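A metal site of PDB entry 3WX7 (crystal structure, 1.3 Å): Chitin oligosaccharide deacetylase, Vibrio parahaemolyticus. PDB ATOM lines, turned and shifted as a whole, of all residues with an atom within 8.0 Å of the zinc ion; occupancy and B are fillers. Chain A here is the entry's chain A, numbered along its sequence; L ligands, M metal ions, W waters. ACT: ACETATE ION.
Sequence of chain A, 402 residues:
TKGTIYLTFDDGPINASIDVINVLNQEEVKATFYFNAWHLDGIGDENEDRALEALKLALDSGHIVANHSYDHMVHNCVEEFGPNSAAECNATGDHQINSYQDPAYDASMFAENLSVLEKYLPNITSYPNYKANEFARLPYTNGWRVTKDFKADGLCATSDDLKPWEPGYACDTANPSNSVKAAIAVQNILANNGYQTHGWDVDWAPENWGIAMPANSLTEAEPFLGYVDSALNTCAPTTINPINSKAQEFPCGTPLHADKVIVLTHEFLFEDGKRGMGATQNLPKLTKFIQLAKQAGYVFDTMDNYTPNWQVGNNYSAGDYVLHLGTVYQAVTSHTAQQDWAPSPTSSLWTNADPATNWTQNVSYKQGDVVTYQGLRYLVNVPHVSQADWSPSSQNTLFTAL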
ATOM      1  N   PHE A   9      -4.685  -7.454 -28.131  1.00  0.00           N
ATOM      2  CA  PHE A   9      -4.038  -8.154 -29.241  1.00  0.00           C
ATOM      3  C   PHE A   9      -3.686  -9.556 -28.768  1.00  0.00           C
ATOM      4  O   PHE A   9      -2.993  -9.697 -27.752  1.00  0.00           O
ATOM      5  CB  PHE A   9      -2.772  -7.418 -29.710  1.00  0.00           C
ATOM      6  CG  PHE A   9      -3.044  -6.078 -30.336  1.00  0.00           C
ATOM      7  CD1 PHE A   9      -3.138  -4.934 -29.564  1.00  0.00           C
ATOM      8  CD2 PHE A   9      -3.187  -5.960 -31.715  1.00  0.00           C
ATOM      9  CE1 PHE A   9      -3.391  -3.695 -30.139  1.00  0.00           C
ATOM     10  CE2 PHE A   9      -3.428  -4.721 -32.283  1.00  0.00           C
ATOM     11  CZ  PHE A   9      -3.531  -3.599 -31.508  1.00  0.00           C
ATOM     12  N   ASP A  10      -4.122 -10.572 -29.502  1.00  0.00           N
ATOM     13  CA  ASP A  10      -3.851 -11.958 -29.162  1.00  0.00           C
ATOM     14  C   ASP A  10      -2.804 -12.591 -30.089  1.00  0.00           C
ATOM     15  O   ASP A  10      -2.732 -12.270 -31.277  1.00  0.00           O
ATOM     16  CB  ASP A  10      -5.129 -12.809 -29.250  1.00  0.00           C
ATOM     17  CG  ASP A  10      -6.064 -12.612 -28.078  1.00  0.00           C
ATOM     18  OD1 ASP A  10      -5.902 -11.675 -27.282  1.00  0.00           O
ATOM     19  OD2 ASP A  10      -7.028 -13.407 -27.972  1.00  0.00           O
ATOM     20  N   ASP A  11      -2.031 -13.504 -29.505  1.00  0.00           N
ATOM     21  CA  ASP A  11      -1.190 -14.510 -30.174  1.00  0.00           C
ATOM     22  C   ASP A  11       0.240 -14.075 -30.463  1.00  0.00           C
ATOM     23  O   ASP A  11       0.986 -14.836 -31.080  1.00  0.00           O
ATOM     24  CB  ASP A  11      -1.831 -15.013 -31.490  1.00  0.00           C
ATOM     25  CG  ASP A  11      -3.144 -15.715 -31.279  1.00  0.00           C
ATOM     26  OD1 ASP A  11      -3.671 -15.621 -30.156  1.00  0.00           O
ATOM     27  OD2 ASP A  11      -3.650 -16.342 -32.233  1.00  0.00           O
ATOM     28  N   GLY A  12       0.634 -12.883 -30.036  1.00  0.00           N
ATOM     29  CA  GLY A  12       2.043 -12.526 -30.075  1.00  0.00           C
ATOM     30  C   GLY A  12       2.833 -13.268 -29.004  1.00  0.00           C
ATOM     31  O   GLY A  12       2.283 -14.125 -28.319  1.00  0.00           O
ATOM     32  N   TYR A  34      -2.197 -10.425 -25.174  1.00  0.00           N
ATOM     33  CA  TYR A  34      -2.373 -11.754 -24.636  1.00  0.00           C
ATOM     34  C   TYR A  34      -1.432 -12.672 -25.403  1.00  0.00           C
ATOM     35  O   TYR A  34      -1.714 -13.076 -26.531  1.00  0.00           O
ATOM     36  CB  TYR A  34      -3.836 -12.204 -24.743  1.00  0.00           C
ATOM     37  CG  TYR A  34      -4.758 -11.515 -23.748  1.00  0.00           C
ATOM     38  CD1 TYR A  34      -5.438 -10.345 -24.091  1.00  0.00           C
ATOM     39  CD2 TYR A  34      -4.930 -12.023 -22.466  1.00  0.00           C
ATOM     40  CE1 TYR A  34      -6.265  -9.712 -23.187  1.00  0.00           C
ATOM     41  CE2 TYR A  34      -5.777 -11.393 -21.554  1.00  0.00           C
ATOM     42  CZ  TYR A  34      -6.421 -10.228 -21.920  1.00  0.00           C
ATOM     43  OH  TYR A  34      -7.260  -9.579 -21.038  1.00  0.00           O
ATOM     44  N   PHE A  35      -0.292 -12.961 -24.783  1.00  0.00           N
ATOM     45  CA  PHE A  35       0.821 -13.602 -25.456  1.00  0.00           C
ATOM     46  C   PHE A  35       0.870 -15.136 -25.292  1.00  0.00           C
ATOM     47  O   PHE A  35       0.447 -15.701 -24.279  1.00  0.00           O
ATOM     48  CB  PHE A  35       2.155 -13.025 -24.938  1.00  0.00           C
ATOM     49  CG  PHE A  35       2.576 -11.713 -25.591  1.00  0.00           C
ATOM     50  CD1 PHE A  35       2.001 -11.229 -26.760  1.00  0.00           C
ATOM     51  CD2 PHE A  35       3.597 -10.974 -25.004  1.00  0.00           C
ATOM     52  CE1 PHE A  35       2.449 -10.044 -27.331  1.00  0.00           C
ATOM     53  CE2 PHE A  35       4.026  -9.776 -25.569  1.00  0.00           C
ATOM     54  CZ  PHE A  35       3.453  -9.314 -26.728  1.00  0.00           C
ATOM     55  N   ASN A  36       1.421 -15.781 -26.325  1.00  0.00           N
ATOM     56  CA  ASN A  36       1.773 -17.199 -26.305  1.00  0.00           C
ATOM     57  C   ASN A  36       3.288 -17.307 -26.438  1.00  0.00           C
ATOM     58  O   ASN A  36       3.838 -17.000 -27.502  1.00  0.00           O
ATOM     59  CB  ASN A  36       1.135 -17.956 -27.483  1.00  0.00           C
ATOM     60  CG  ASN A  36      -0.374 -17.762 -27.573  1.00  0.00           C
ATOM     61  OD1 ASN A  36      -0.878 -17.230 -28.572  1.00  0.00           O
ATOM     62  ND2 ASN A  36      -1.096 -18.218 -26.551  1.00  0.00           N
ATOM     63  N   HIS A  68      -2.038 -15.879 -22.483  1.00  0.00           N
ATOM     64  CA  HIS A  68      -2.896 -16.549 -23.468  1.00  0.00           C
ATOM     65  C   HIS A  68      -2.539 -18.041 -23.598  1.00  0.00           C
ATOM     66  O   HIS A  68      -3.038 -18.712 -24.520  1.00  0.00           O
ATOM     67  CB  HIS A  68      -2.781 -15.840 -24.817  1.00  0.00           C
ATOM     68  CG  HIS A  68      -3.892 -16.106 -25.781  1.00  0.00           C
ATOM     69  ND1 HIS A  68      -5.211 -16.300 -25.393  1.00  0.00           N
ATOM     70  CD2 HIS A  68      -3.878 -16.163 -27.128  1.00  0.00           C
ATOM     71  CE1 HIS A  68      -5.946 -16.470 -26.475  1.00  0.00           C
ATOM     72  NE2 HIS A  68      -5.167 -16.389 -27.541  1.00  0.00           N
ATOM     73  N   SER A  69      -1.674 -18.526 -22.691  1.00  0.00           N
ATOM     74  CA  SER A  69      -1.125 -19.911 -22.605  1.00  0.00           C
ATOM     75  C   SER A  69       0.114 -20.075 -23.473  1.00  0.00           C
ATOM     76  O   SER A  69       0.317 -19.351 -24.443  1.00  0.00           O
ATOM     77  CB  SER A  69      -2.175 -20.992 -22.964  1.00  0.00           C
ATOM     78  OG  SER A  69      -2.265 -21.200 -24.376  1.00  0.00           O
ATOM     79  N   HIS A  72      -1.083 -21.947 -27.169  1.00  0.00           N
ATOM     80  CA  HIS A  72      -2.403 -21.709 -27.784  1.00  0.00           C
ATOM     81  C   HIS A  72      -3.225 -23.003 -27.855  1.00  0.00           C
ATOM     82  O   HIS A  72      -4.073 -23.144 -28.736  1.00  0.00           O
ATOM     83  CB  HIS A  72      -2.237 -21.114 -29.187  1.00  0.00           C
ATOM     84  CG  HIS A  72      -3.389 -20.261 -29.600  1.00  0.00           C
ATOM     85  ND1 HIS A  72      -4.563 -20.774 -30.117  1.00  0.00           N
ATOM     86  CD2 HIS A  72      -3.559 -18.933 -29.526  1.00  0.00           C
ATOM     87  CE1 HIS A  72      -5.400 -19.791 -30.350  1.00  0.00           C
ATOM     88  NE2 HIS A  72      -4.818 -18.657 -30.011  1.00  0.00           N
ATOM     89  N   ARG A 137      -6.721 -15.031 -21.024  1.00  0.00           N
ATOM     90  CA  ARG A 137      -7.792 -15.208 -21.999  1.00  0.00           C
ATOM     91  C   ARG A 137      -7.579 -16.583 -22.611  1.00  0.00           C
ATOM     92  O   ARG A 137      -6.453 -16.906 -23.011  1.00  0.00           O
ATOM     93  CB  ARG A 137      -7.769 -14.102 -23.056  1.00  0.00           C
ATOM     94  CG  ARG A 137      -8.799 -14.314 -24.171  1.00  0.00           C
ATOM     95  CD  ARG A 137      -8.735 -13.185 -25.154  1.00  0.00           C
ATOM     96  NE  ARG A 137      -9.335 -11.961 -24.632  1.00  0.00           N
ATOM     97  CZ  ARG A 137      -9.147 -10.749 -25.166  1.00  0.00           C
ATOM     98  NH1 ARG A 137      -8.307 -10.587 -26.192  1.00  0.00           N
ATOM     99  NH2 ARG A 137      -9.769  -9.705 -24.653  1.00  0.00           N
ATOM    100  N   LEU A 138      -8.627 -17.398 -22.648  1.00  0.00           N
ATOM    101  CA  LEU A 138      -8.508 -18.730 -23.246  1.00  0.00           C
ATOM    102  C   LEU A 138      -8.481 -18.684 -24.767  1.00  0.00           C
ATOM    103  O   LEU A 138      -9.327 -18.026 -25.387  1.00  0.00           O
ATOM    104  CB  LEU A 138      -9.643 -19.628 -22.788  1.00  0.00           C
ATOM    105  CG  LEU A 138      -9.370 -20.517 -21.574  1.00  0.00           C
ATOM    106  CD1 LEU A 138      -9.170 -19.680 -20.307  1.00  0.00           C
ATOM    107  CD2 LEU A 138     -10.486 -21.531 -21.382  1.00  0.00           C
ATOM    108  N   PRO A 139      -7.539 -19.401 -25.390  1.00  0.00           N
ATOM    109  CA  PRO A 139      -7.620 -19.631 -26.836  1.00  0.00           C
ATOM    110  C   PRO A 139      -9.029 -20.034 -27.298  1.00  0.00           C
ATOM    111  O   PRO A 139      -9.689 -20.853 -26.648  1.00  0.00           O
ATOM    112  CB  PRO A 139      -6.605 -20.771 -27.050  1.00  0.00           C
ATOM    113  CG  PRO A 139      -5.559 -20.465 -26.023  1.00  0.00           C
ATOM    114  CD  PRO A 139      -6.348 -20.035 -24.802  1.00  0.00           C
ATOM    115  N   TYR A 140      -9.486 -19.379 -28.368  1.00  0.00           N
ATOM    116  CA  TYR A 140     -10.737 -19.664 -29.097  1.00  0.00           C
ATOM    117  C   TYR A 140     -12.040 -19.285 -28.389  1.00  0.00           C
ATOM    118  O   TYR A 140     -13.118 -19.419 -28.955  1.00  0.00           O
ATOM    119  CB  TYR A 140     -10.823 -21.161 -29.463  1.00  0.00           C
ATOM    120  CG  TYR A 140      -9.518 -21.753 -29.922  1.00  0.00           C
ATOM    121  CD1 TYR A 140      -8.912 -21.302 -31.074  1.00  0.00           C
ATOM    122  CD2 TYR A 140      -8.895 -22.763 -29.194  1.00  0.00           C
ATOM    123  CE1 TYR A 140      -7.715 -21.824 -31.493  1.00  0.00           C
ATOM    124  CE2 TYR A 140      -7.677 -23.280 -29.607  1.00  0.00           C
ATOM    125  CZ  TYR A 140      -7.111 -22.820 -30.758  1.00  0.00           C
ATOM    126  OH  TYR A 140      -5.899 -23.349 -31.177  1.00  0.00           O
ATOM    127  N   THR A 141     -11.952 -18.793 -27.161  1.00  0.00           N
ATOM    128  CA  THR A 141     -13.092 -18.850 -26.275  1.00  0.00           C
ATOM    129  C   THR A 141     -13.447 -17.509 -25.639  1.00  0.00           C
ATOM    130  O   THR A 141     -12.617 -16.919 -24.937  1.00  0.00           O
ATOM    131  CB  THR A 141     -12.800 -19.867 -25.162  1.00  0.00           C
ATOM    132  OG1 THR A 141     -12.433 -21.107 -25.773  1.00  0.00           O
ATOM    133  CG2 THR A 141     -14.014 -20.093 -24.277  1.00  0.00           C
ATOM    134  N   TRP A 200     -14.268 -10.781 -25.143  1.00  0.00           N
ATOM    135  CA  TRP A 200     -14.279  -9.580 -25.981  1.00  0.00           C
ATOM    136  C   TRP A 200     -15.687  -9.227 -26.439  1.00  0.00           C
ATOM    137  O   TRP A 200     -16.583 -10.069 -26.417  1.00  0.00           O
ATOM    138  CB  TRP A 200     -13.351  -9.735 -27.200  1.00  0.00           C
ATOM    139  CG  TRP A 200     -13.714 -10.902 -28.106  1.00  0.00           C
ATOM    140  CD1 TRP A 200     -14.500 -10.857 -29.222  1.00  0.00           C
ATOM    141  CD2 TRP A 200     -13.330 -12.274 -27.951  1.00  0.00           C
ATOM    142  NE1 TRP A 200     -14.615 -12.105 -29.783  1.00  0.00           N
ATOM    143  CE2 TRP A 200     -13.896 -12.996 -29.021  1.00  0.00           C
ATOM    144  CE3 TRP A 200     -12.524 -12.951 -27.029  1.00  0.00           C
ATOM    145  CZ2 TRP A 200     -13.707 -14.369 -29.177  1.00  0.00           C
ATOM    146  CZ3 TRP A 200     -12.354 -14.312 -27.192  1.00  0.00           C
ATOM    147  CH2 TRP A 200     -12.926 -15.005 -28.265  1.00  0.00           C
ATOM    148  N   LEU A 264     -10.975  -7.322 -29.632  1.00  0.00           N
ATOM    149  CA  LEU A 264     -10.001  -8.367 -29.918  1.00  0.00           C
ATOM    150  C   LEU A 264      -9.464  -8.194 -31.324  1.00  0.00           C
ATOM    151  O   LEU A 264     -10.247  -7.968 -32.259  1.00  0.00           O
ATOM    152  CB  LEU A 264     -10.634  -9.747 -29.789  1.00  0.00           C
ATOM    153  CG  LEU A 264      -9.886 -10.908 -30.453  1.00  0.00           C
ATOM    154  CD1 LEU A 264      -8.579 -11.204 -29.725  1.00  0.00           C
ATOM    155  CD2 LEU A 264     -10.764 -12.127 -30.507  1.00  0.00           C
ATOM    156  N   THR A 265      -8.157  -8.272 -31.486  1.00  0.00           N
ATOM    157  CA  THR A 265      -7.580  -8.483 -32.812  1.00  0.00           C
ATOM    158  C   THR A 265      -6.239  -9.206 -32.648  1.00  0.00           C
ATOM    159  O   THR A 265      -5.908  -9.687 -31.562  1.00  0.00           O
ATOM    160  CB  THR A 265      -7.462  -7.158 -33.589  1.00  0.00           C
ATOM    161  OG1 THR A 265      -7.140  -7.420 -34.964  1.00  0.00           O
ATOM    162  CG2 THR A 265      -6.429  -6.219 -32.987  1.00  0.00           C
ATOM    163  N   HIS A 266      -5.488  -9.335 -33.741  1.00  0.00           N
ATOM    164  CA  HIS A 266      -4.260 -10.115 -33.759  1.00  0.00           C
ATOM    165  C   HIS A 266      -3.207  -9.348 -34.534  1.00  0.00           C
ATOM    166  O   HIS A 266      -3.483  -8.885 -35.650  1.00  0.00           O
ATOM    167  CB  HIS A 266      -4.477 -11.482 -34.417  1.00  0.00           C
ATOM    168  CG  HIS A 266      -5.511 -12.319 -33.756  1.00  0.00           C
ATOM    169  ND1 HIS A 266      -6.869 -12.185 -33.996  1.00  0.00           N
ATOM    170  CD2 HIS A 266      -5.393 -13.335 -32.857  1.00  0.00           C
ATOM    171  CE1 HIS A 266      -7.527 -13.072 -33.275  1.00  0.00           C
ATOM    172  NE2 HIS A 266      -6.660 -13.770 -32.574  1.00  0.00           N
ATOM    173  N   PHE A 268      -0.861 -10.457 -36.210  1.00  0.00           N
ATOM    174  CA  PHE A 268      -0.526 -11.078 -37.500  1.00  0.00           C
ATOM    175  C   PHE A 268      -1.412 -10.539 -38.639  1.00  0.00           C
ATOM    176  O   PHE A 268      -1.092 -10.746 -39.813  1.00  0.00           O
ATOM    177  CB  PHE A 268      -0.575 -12.620 -37.422  1.00  0.00           C
ATOM    178  CG  PHE A 268      -1.918 -13.228 -37.062  1.00  0.00           C
ATOM    179  CD1 PHE A 268      -3.043 -13.052 -37.864  1.00  0.00           C
ATOM    180  CD2 PHE A 268      -2.026 -14.067 -35.957  1.00  0.00           C
ATOM    181  CE1 PHE A 268      -4.246 -13.643 -37.526  1.00  0.00           C
ATOM    182  CE2 PHE A 268      -3.217 -14.660 -35.627  1.00  0.00           C
ATOM    183  CZ  PHE A 268      -4.335 -14.453 -36.411  1.00  0.00           C
HETATM  184  C   ACT L   1      -8.147 -16.107 -29.248  1.00  0.00           C
HETATM  185  O   ACT L   1      -7.838 -17.348 -29.280  1.00  0.00           O
HETATM  186  OXT ACT L   1      -7.326 -15.277 -29.736  1.00  0.00           O
HETATM  187  CH3 ACT L   1      -9.431 -15.641 -28.635  1.00  0.00           C
HETATM  188 ZN    ZN M   1      -5.549 -16.664 -29.688  1.00  0.00          ZN
HETATM  189  O   HOH W   1      -6.171 -16.576 -31.918  1.00  0.00           O
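NH1 of Arg 137 lies within salt-bridge range of OD1 of Asp 10 (2.9 Å). The backbone carbonyl oxygen of His 68 is in hydrogen-bond range of the side-chain amide nitrogen of Asn 36 (2.9 Å). ND1 of His 68 sits at hydrogen-bond distance from O of Arg 137, 2.8 Å away. N of His 68 lies within hydrogen-bond range of O of Phe 35. The backbone NH (N) of Asp 11 is in hydrogen-bond range of the backbone carbonyl oxygen (O) of Tyr 34 (3.0 Å). The backbone NH of His 72 sits at hydrogen-bond distance from the side-chain hydroxyl of Ser 69. O of His 72 sits at hydrogen-bond distance from OH of Tyr 140. The backbone NH (N) of Asp 10 is in hydrogen-bond range of the backbone carbonyl oxygen (O) of Thr 265 (2.9 Å).
CB of Asp 10 touches the zinc ion, 3.9 Å away. Of the 20 residues printed, 4 come within 4 Å of the zinc ion.
The zinc ion is bound by a ring nitrogen (NE2) of His 72, a ring nitrogen (NE2) of His 68, the side-chain carboxylate (OD1) of Asp 11, an oxygen (OXT) of the ligand, water W1 and an oxygen (O) of the ligand. The zinc ion has six donor atoms within binding distance.
Water W1 bridges the side-chain carboxylate (OD2) of Asp 11 (2.6 Å) and a ring nitrogen (NE2) of His 266 (2.9 Å).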
